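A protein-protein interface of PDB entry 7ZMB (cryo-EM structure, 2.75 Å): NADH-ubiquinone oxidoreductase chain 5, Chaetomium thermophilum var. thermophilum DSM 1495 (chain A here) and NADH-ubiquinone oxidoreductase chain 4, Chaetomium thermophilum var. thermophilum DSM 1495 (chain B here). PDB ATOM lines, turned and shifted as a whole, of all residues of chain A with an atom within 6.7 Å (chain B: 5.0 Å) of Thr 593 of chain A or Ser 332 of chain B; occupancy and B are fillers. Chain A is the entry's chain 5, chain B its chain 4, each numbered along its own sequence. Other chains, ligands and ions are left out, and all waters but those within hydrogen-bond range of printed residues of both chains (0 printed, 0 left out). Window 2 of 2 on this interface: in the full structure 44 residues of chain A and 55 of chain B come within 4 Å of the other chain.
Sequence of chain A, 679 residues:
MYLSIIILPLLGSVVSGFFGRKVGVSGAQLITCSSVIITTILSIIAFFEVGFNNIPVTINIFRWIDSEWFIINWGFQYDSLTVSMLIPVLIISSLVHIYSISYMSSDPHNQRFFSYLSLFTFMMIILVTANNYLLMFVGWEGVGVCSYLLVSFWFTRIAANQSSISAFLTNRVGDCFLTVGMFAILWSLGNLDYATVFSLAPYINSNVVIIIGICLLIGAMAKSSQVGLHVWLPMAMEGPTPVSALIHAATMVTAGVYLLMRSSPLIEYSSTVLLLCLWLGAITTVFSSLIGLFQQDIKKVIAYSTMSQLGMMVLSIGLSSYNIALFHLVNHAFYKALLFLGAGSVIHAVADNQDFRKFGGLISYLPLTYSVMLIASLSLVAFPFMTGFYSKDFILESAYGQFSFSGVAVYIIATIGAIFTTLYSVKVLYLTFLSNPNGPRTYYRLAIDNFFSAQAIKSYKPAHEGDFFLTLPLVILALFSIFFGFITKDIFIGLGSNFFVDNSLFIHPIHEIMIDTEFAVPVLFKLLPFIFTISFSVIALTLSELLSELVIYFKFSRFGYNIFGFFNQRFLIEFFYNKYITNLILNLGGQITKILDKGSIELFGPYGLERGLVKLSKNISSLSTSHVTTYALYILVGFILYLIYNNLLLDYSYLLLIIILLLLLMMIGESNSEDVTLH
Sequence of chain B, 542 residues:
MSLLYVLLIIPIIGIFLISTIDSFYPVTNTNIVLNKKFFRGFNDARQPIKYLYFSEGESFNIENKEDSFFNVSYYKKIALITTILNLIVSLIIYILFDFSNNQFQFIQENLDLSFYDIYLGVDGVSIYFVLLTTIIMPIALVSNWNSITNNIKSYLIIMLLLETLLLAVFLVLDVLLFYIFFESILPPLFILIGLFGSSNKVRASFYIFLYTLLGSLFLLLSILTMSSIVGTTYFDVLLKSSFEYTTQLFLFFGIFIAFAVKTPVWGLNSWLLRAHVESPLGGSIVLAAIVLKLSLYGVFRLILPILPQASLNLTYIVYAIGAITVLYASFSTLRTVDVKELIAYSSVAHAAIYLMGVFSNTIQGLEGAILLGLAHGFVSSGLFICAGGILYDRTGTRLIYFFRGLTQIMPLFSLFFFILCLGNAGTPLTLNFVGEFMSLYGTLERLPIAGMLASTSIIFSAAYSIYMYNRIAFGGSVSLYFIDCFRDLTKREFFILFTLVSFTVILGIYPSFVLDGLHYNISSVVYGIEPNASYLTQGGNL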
ATOM      1  N   LEU A 588     -29.442  -8.544  -1.269  1.00  0.00           N
ATOM      2  CA  LEU A 588     -30.034  -7.743  -2.337  1.00  0.00           C
ATOM      3  C   LEU A 588     -29.257  -6.455  -2.550  1.00  0.00           C
ATOM      4  O   LEU A 588     -28.999  -6.062  -3.692  1.00  0.00           O
ATOM      5  CB  LEU A 588     -31.507  -7.449  -2.055  1.00  0.00           C
ATOM      6  CG  LEU A 588     -32.557  -8.484  -2.441  1.00  0.00           C
ATOM      7  CD1 LEU A 588     -32.551  -8.627  -3.937  1.00  0.00           C
ATOM      8  CD2 LEU A 588     -32.281  -9.824  -1.836  1.00  0.00           C
ATOM      9  N   GLY A 589     -28.861  -5.793  -1.466  1.00  0.00           N
ATOM     10  CA  GLY A 589     -27.951  -4.675  -1.600  1.00  0.00           C
ATOM     11  C   GLY A 589     -26.644  -5.068  -2.247  1.00  0.00           C
ATOM     12  O   GLY A 589     -26.075  -4.296  -3.020  1.00  0.00           O
ATOM     13  N   GLY A 590     -26.153  -6.271  -1.943  1.00  0.00           N
ATOM     14  CA  GLY A 590     -24.928  -6.742  -2.563  1.00  0.00           C
ATOM     15  C   GLY A 590     -25.078  -7.017  -4.046  1.00  0.00           C
ATOM     16  O   GLY A 590     -24.180  -6.714  -4.834  1.00  0.00           O
ATOM     17  N   GLN A 591     -26.203  -7.616  -4.447  1.00  0.00           N
ATOM     18  CA  GLN A 591     -26.446  -7.862  -5.866  1.00  0.00           C
ATOM     19  C   GLN A 591     -26.588  -6.556  -6.642  1.00  0.00           C
ATOM     20  O   GLN A 591     -26.052  -6.420  -7.746  1.00  0.00           O
ATOM     21  CB  GLN A 591     -27.693  -8.722  -6.051  1.00  0.00           C
ATOM     22  CG  GLN A 591     -27.572 -10.130  -5.517  1.00  0.00           C
ATOM     23  CD  GLN A 591     -26.852 -11.057  -6.475  1.00  0.00           C
ATOM     24  OE1 GLN A 591     -25.710 -11.449  -6.237  1.00  0.00           O
ATOM     25  NE2 GLN A 591     -27.521 -11.417  -7.566  1.00  0.00           N
ATOM     26  N   ILE A 592     -27.309  -5.584  -6.076  1.00  0.00           N
ATOM     27  CA  ILE A 592     -27.577  -4.337  -6.786  1.00  0.00           C
ATOM     28  C   ILE A 592     -26.298  -3.538  -6.975  1.00  0.00           C
ATOM     29  O   ILE A 592     -26.063  -2.963  -8.041  1.00  0.00           O
ATOM     30  CB  ILE A 592     -28.640  -3.513  -6.039  1.00  0.00           C
ATOM     31  CG1 ILE A 592     -29.996  -4.190  -6.102  1.00  0.00           C
ATOM     32  CG2 ILE A 592     -28.761  -2.121  -6.626  1.00  0.00           C
ATOM     33  CD1 ILE A 592     -30.932  -3.697  -5.040  1.00  0.00           C
ATOM     34  N   THR A 593     -25.452  -3.481  -5.952  1.00  0.00           N
ATOM     35  CA  THR A 593     -24.305  -2.588  -5.993  1.00  0.00           C
ATOM     36  C   THR A 593     -23.076  -3.212  -6.638  1.00  0.00           C
ATOM     37  O   THR A 593     -22.078  -2.512  -6.828  1.00  0.00           O
ATOM     38  CB  THR A 593     -23.961  -2.107  -4.578  1.00  0.00           C
ATOM     39  OG1 THR A 593     -23.120  -0.954  -4.660  1.00  0.00           O
ATOM     40  CG2 THR A 593     -23.250  -3.195  -3.792  1.00  0.00           C
ATOM     41  N   LYS A 594     -23.120  -4.499  -6.980  1.00  0.00           N
ATOM     42  CA  LYS A 594     -22.030  -5.167  -7.684  1.00  0.00           C
ATOM     43  C   LYS A 594     -22.406  -5.556  -9.102  1.00  0.00           C
ATOM     44  O   LYS A 594     -21.710  -5.189 -10.048  1.00  0.00           O
ATOM     45  CB  LYS A 594     -21.573  -6.410  -6.912  1.00  0.00           C
ATOM     46  CG  LYS A 594     -21.149  -6.137  -5.489  1.00  0.00           C
ATOM     47  CD  LYS A 594     -20.449  -7.342  -4.884  1.00  0.00           C
ATOM     48  CE  LYS A 594     -21.234  -7.920  -3.728  1.00  0.00           C
ATOM     49  NZ  LYS A 594     -20.594  -9.133  -3.180  1.00  0.00           N
ATOM     50  N   ILE A 595     -23.494  -6.304  -9.272  1.00  0.00           N
ATOM     51  CA  ILE A 595     -23.942  -6.677 -10.607  1.00  0.00           C
ATOM     52  C   ILE A 595     -24.528  -5.475 -11.347  1.00  0.00           C
ATOM     53  O   ILE A 595     -24.297  -5.304 -12.545  1.00  0.00           O
ATOM     54  CB  ILE A 595     -24.947  -7.847 -10.540  1.00  0.00           C
ATOM     55  CG1 ILE A 595     -24.295  -9.106  -9.972  1.00  0.00           C
ATOM     56  CG2 ILE A 595     -25.534  -8.138 -11.905  1.00  0.00           C
ATOM     57  CD1 ILE A 595     -24.449  -9.275  -8.489  1.00  0.00           C
ATOM     58  N   LEU A 596     -25.302  -4.630 -10.668  1.00  0.00           N
ATOM     59  CA  LEU A 596     -26.020  -3.565 -11.380  1.00  0.00           C
ATOM     60  C   LEU A 596     -25.229  -2.262 -11.425  1.00  0.00           C
ATOM     61  O   LEU A 596     -24.777  -1.851 -12.495  1.00  0.00           O
ATOM     62  CB  LEU A 596     -27.397  -3.338 -10.754  1.00  0.00           C
ATOM     63  CG  LEU A 596     -28.345  -4.532 -10.734  1.00  0.00           C
ATOM     64  CD1 LEU A 596     -29.717  -4.069 -10.329  1.00  0.00           C
ATOM     65  CD2 LEU A 596     -28.379  -5.203 -12.089  1.00  0.00           C
ATOM     66  N   ASP A 597     -25.007  -1.638 -10.270  1.00  0.00           N
ATOM     67  CA  ASP A 597     -24.449  -0.291 -10.250  1.00  0.00           C
ATOM     68  C   ASP A 597     -23.043  -0.258 -10.817  1.00  0.00           C
ATOM     69  O   ASP A 597     -22.809   0.322 -11.882  1.00  0.00           O
ATOM     70  CB  ASP A 597     -24.421   0.280  -8.836  1.00  0.00           C
ATOM     71  CG  ASP A 597     -25.790   0.609  -8.311  1.00  0.00           C
ATOM     72  OD1 ASP A 597     -26.782   0.251  -8.966  1.00  0.00           O
ATOM     73  OD2 ASP A 597     -25.873   1.266  -7.257  1.00  0.00           O
ATOM     74  N   LYS A 598     -22.104  -0.893 -10.127  1.00  0.00           N
ATOM     75  CA  LYS A 598     -20.745  -1.030 -10.638  1.00  0.00           C
ATOM     76  C   LYS A 598     -20.643  -2.256 -11.532  1.00  0.00           C
ATOM     77  O   LYS A 598     -19.727  -3.066 -11.431  1.00  0.00           O
ATOM     78  CB  LYS A 598     -19.771  -1.117  -9.472  1.00  0.00           C
ATOM     79  CG  LYS A 598     -19.613   0.171  -8.689  1.00  0.00           C
ATOM     80  CD  LYS A 598     -19.362  -0.109  -7.220  1.00  0.00           C
ATOM     81  CE  LYS A 598     -19.052   1.162  -6.465  1.00  0.00           C
ATOM     82  NZ  LYS A 598     -19.749   2.341  -7.046  1.00  0.00           N
ATOM     83  N   GLY A 599     -21.613  -2.372 -12.434  1.00  0.00           N
ATOM     84  CA  GLY A 599     -21.827  -3.558 -13.238  1.00  0.00           C
ATOM     85  C   GLY A 599     -22.418  -3.280 -14.601  1.00  0.00           C
ATOM     86  O   GLY A 599     -21.878  -2.512 -15.400  1.00  0.00           O
ATOM     87  N   TYR B 328     -34.145   0.467  -4.510  1.00  0.00           N
ATOM     88  CA  TYR B 328     -32.797   0.066  -4.895  1.00  0.00           C
ATOM     89  C   TYR B 328     -31.744   1.000  -4.320  1.00  0.00           C
ATOM     90  O   TYR B 328     -30.657   0.555  -3.941  1.00  0.00           O
ATOM     91  CB  TYR B 328     -32.653   0.037  -6.412  1.00  0.00           C
ATOM     92  CG  TYR B 328     -33.454  -1.028  -7.089  1.00  0.00           C
ATOM     93  CD1 TYR B 328     -34.019  -2.070  -6.366  1.00  0.00           C
ATOM     94  CD2 TYR B 328     -33.583  -1.042  -8.463  1.00  0.00           C
ATOM     95  CE1 TYR B 328     -34.747  -3.054  -6.990  1.00  0.00           C
ATOM     96  CE2 TYR B 328     -34.296  -2.026  -9.091  1.00  0.00           C
ATOM     97  CZ  TYR B 328     -34.880  -3.026  -8.351  1.00  0.00           C
ATOM     98  OH  TYR B 328     -35.592  -4.007  -8.989  1.00  0.00           O
ATOM     99  N   ALA B 329     -32.031   2.299  -4.278  1.00  0.00           N
ATOM    100  CA  ALA B 329     -31.056   3.241  -3.751  1.00  0.00           C
ATOM    101  C   ALA B 329     -30.892   3.123  -2.246  1.00  0.00           C
ATOM    102  O   ALA B 329     -29.953   3.703  -1.699  1.00  0.00           O
ATOM    103  CB  ALA B 329     -31.427   4.675  -4.129  1.00  0.00           C
ATOM    104  N   SER B 330     -31.774   2.394  -1.569  1.00  0.00           N
ATOM    105  CA  SER B 330     -31.621   2.149  -0.144  1.00  0.00           C
ATOM    106  C   SER B 330     -30.782   0.912   0.134  1.00  0.00           C
ATOM    107  O   SER B 330     -29.928   0.934   1.023  1.00  0.00           O
ATOM    108  CB  SER B 330     -32.992   2.013   0.512  1.00  0.00           C
ATOM    109  OG  SER B 330     -33.796   3.142   0.235  1.00  0.00           O
ATOM    110  N   PHE B 331     -30.995  -0.159  -0.633  1.00  0.00           N
ATOM    111  CA  PHE B 331     -30.244  -1.395  -0.430  1.00  0.00           C
ATOM    112  C   PHE B 331     -28.771  -1.217  -0.745  1.00  0.00           C
ATOM    113  O   PHE B 331     -27.913  -1.733  -0.025  1.00  0.00           O
ATOM    114  CB  PHE B 331     -30.827  -2.515  -1.287  1.00  0.00           C
ATOM    115  CG  PHE B 331     -32.266  -2.790  -1.029  1.00  0.00           C
ATOM    116  CD1 PHE B 331     -32.880  -2.354   0.129  1.00  0.00           C
ATOM    117  CD2 PHE B 331     -33.014  -3.489  -1.952  1.00  0.00           C
ATOM    118  CE1 PHE B 331     -34.204  -2.604   0.354  1.00  0.00           C
ATOM    119  CE2 PHE B 331     -34.342  -3.742  -1.722  1.00  0.00           C
ATOM    120  CZ  PHE B 331     -34.930  -3.302  -0.560  1.00  0.00           C
ATOM    121  N   SER B 332     -28.454  -0.505  -1.826  1.00  0.00           N
ATOM    122  CA  SER B 332     -27.054  -0.297  -2.173  1.00  0.00           C
ATOM    123  C   SER B 332     -26.352   0.594  -1.157  1.00  0.00           C
ATOM    124  O   SER B 332     -25.231   0.295  -0.736  1.00  0.00           O
ATOM    125  CB  SER B 332     -26.936   0.293  -3.574  1.00  0.00           C
ATOM    126  OG  SER B 332     -27.012  -0.706  -4.563  1.00  0.00           O
ATOM    127  N   THR B 333     -26.993   1.687  -0.743  1.00  0.00           N
ATOM    128  CA  THR B 333     -26.368   2.550   0.252  1.00  0.00           C
ATOM    129  C   THR B 333     -26.231   1.838   1.589  1.00  0.00           C
ATOM    130  O   THR B 333     -25.458   2.274   2.449  1.00  0.00           O
ATOM    131  CB  THR B 333     -27.149   3.863   0.393  1.00  0.00           C
ATOM    132  OG1 THR B 333     -26.372   4.814   1.122  1.00  0.00           O
ATOM    133  CG2 THR B 333     -28.418   3.651   1.108  1.00  0.00           C
ATOM    134  N   LEU B 334     -26.951   0.734   1.778  1.00  0.00           N
ATOM    135  CA  LEU B 334     -26.713  -0.099   2.950  1.00  0.00           C
ATOM    136  C   LEU B 334     -25.366  -0.811   2.860  1.00  0.00           C
ATOM    137  O   LEU B 334     -24.741  -1.099   3.884  1.00  0.00           O
ATOM    138  CB  LEU B 334     -27.855  -1.100   3.117  1.00  0.00           C
ATOM    139  CG  LEU B 334     -27.907  -1.865   4.441  1.00  0.00           C
ATOM    140  CD1 LEU B 334     -28.034  -0.933   5.638  1.00  0.00           C
ATOM    141  CD2 LEU B 334     -29.039  -2.865   4.417  1.00  0.00           C
ATOM    142  N   ARG B 335     -24.897  -1.091   1.643  1.00  0.00           N
ATOM    143  CA  ARG B 335     -23.660  -1.831   1.416  1.00  0.00           C
ATOM    144  C   ARG B 335     -22.489  -0.944   0.998  1.00  0.00           C
ATOM    145  O   ARG B 335     -21.448  -1.467   0.598  1.00  0.00           O
ATOM    146  CB  ARG B 335     -23.878  -2.907   0.351  1.00  0.00           C
ATOM    147  CG  ARG B 335     -24.662  -4.115   0.810  1.00  0.00           C
ATOM    148  CD  ARG B 335     -23.983  -4.847   1.959  1.00  0.00           C
ATOM    149  NE  ARG B 335     -22.670  -5.373   1.613  1.00  0.00           N
ATOM    150  CZ  ARG B 335     -22.457  -6.559   1.056  1.00  0.00           C
ATOM    151  NH1 ARG B 335     -23.473  -7.358   0.759  1.00  0.00           N
ATOM    152  NH2 ARG B 335     -21.222  -6.948   0.789  1.00  0.00           N
ATOM    153  N   THR B 336     -22.628   0.373   1.074  1.00  0.00           N
ATOM    154  CA  THR B 336     -21.603   1.273   0.560  1.00  0.00           C
ATOM    155  C   THR B 336     -20.477   1.454   1.575  1.00  0.00           C
ATOM    156  O   THR B 336     -20.721   1.660   2.766  1.00  0.00           O
ATOM    157  CB  THR B 336     -22.225   2.626   0.200  1.00  0.00           C
ATOM    158  OG1 THR B 336     -22.955   2.505  -1.024  1.00  0.00           O
ATOM    159  CG2 THR B 336     -21.159   3.678   0.002  1.00  0.00           C
ATOM    160  N   TYR B 345     -25.494   8.821  -1.955  1.00  0.00           N
ATOM    161  CA  TYR B 345     -26.458   7.943  -2.585  1.00  0.00           C
ATOM    162  C   TYR B 345     -27.732   7.800  -1.765  1.00  0.00           C
ATOM    163  O   TYR B 345     -28.721   7.264  -2.268  1.00  0.00           O
ATOM    164  CB  TYR B 345     -25.770   6.608  -2.872  1.00  0.00           C
ATOM    165  CG  TYR B 345     -26.579   5.564  -3.580  1.00  0.00           C
ATOM    166  CD1 TYR B 345     -26.837   5.682  -4.931  1.00  0.00           C
ATOM    167  CD2 TYR B 345     -26.915   4.391  -2.967  1.00  0.00           C
ATOM    168  CE1 TYR B 345     -27.527   4.731  -5.611  1.00  0.00           C
ATOM    169  CE2 TYR B 345     -27.600   3.423  -3.646  1.00  0.00           C
ATOM    170  CZ  TYR B 345     -27.893   3.594  -4.978  1.00  0.00           C
ATOM    171  OH  TYR B 345     -28.573   2.633  -5.682  1.00  0.00           O
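The side-chain carboxylate of Asp 597 of chain A lies within hydrogen-bond range of the side-chain hydroxyl of Tyr 345 of chain B (3.4 Å).
OG of Ser 332 of chain B lies close to N of Thr 593 of chain A, 3.5 Å away.
O of Ile 592 of chain A is in hydrogen-bond range of N of Asp 597 of chain A (2.8 Å).
The side-chain hydroxyl (OG1) of Thr 336 of chain B lies within hydrogen-bond range of the backbone carbonyl oxygen (O) of Ser 332 of chain B (3.2 Å).
The side-chain hydroxyl of Tyr 345 of chain B lies within hydrogen-bond range of the backbone carbonyl oxygen of Tyr 328 of chain B (3.4 Å).
Among the printed residues, merely in contact across the chains: Gly 589 of chain A with Phe 331 of chain B (3.3 Å), Gly 589 of chain A with Arg 335 of chain B (3.8 Å), Gly 590 of chain A with Arg 335 of chain B (3.7 Å), Ile 592 of chain A with Tyr 328 of chain B (3.7 Å), Ile 592 of chain A with Phe 331 of chain B (3.7 Å), Ile 592 of chain A with Ser 332 of chain B (3.1 Å) and Asp 597 of chain A with Ser 332 of chain B (3.5 Å).
Of the printed residues of chain B, Gly 589 of chain A touches Phe 331 and Arg 335.
Of the printed residues of chain B, Ile 592 of chain A touches Tyr 328 (3.7 Å), Phe 331 (3.7 Å) and Ser 332 (3.1 Å).
Thr 593 of chain A touches just one residue of chain B: Ser 332 (3.4 Å).
Of the printed residues of chain B, Asp 597 of chain A touches Ser 332 (3.5 Å) and Tyr 345 (3.4 Å).
Printed residues of chain A within 4 Å of Ser 332 of chain B: Ile 592 (3.1 Å), Thr 593 (3.4 Å) and Asp 597 (3.5 Å).
Leu 334 of chain B touches none of the printed residues of chain A.
Of the printed residues of chain A, Arg 335 of chain B touches Gly 589 (3.8 Å) and Gly 590 (3.7 Å).
The nearest printed residue of chain A that does not touch Ser 332 of chain B is Gly 589 of chain A (4.02 Å).
Of the 12 printed residues of chain A, 5 touch a printed residue of chain B.
Printed residues of chain A that touch a printed residue of chain B: Gly 589, Gly 590, Ile 592, Thr 593 and Asp 597.
Hydrophobic or aromatic side chains of chain B that line the printed part of chain A: Tyr 328, Phe 331 and Tyr 345.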
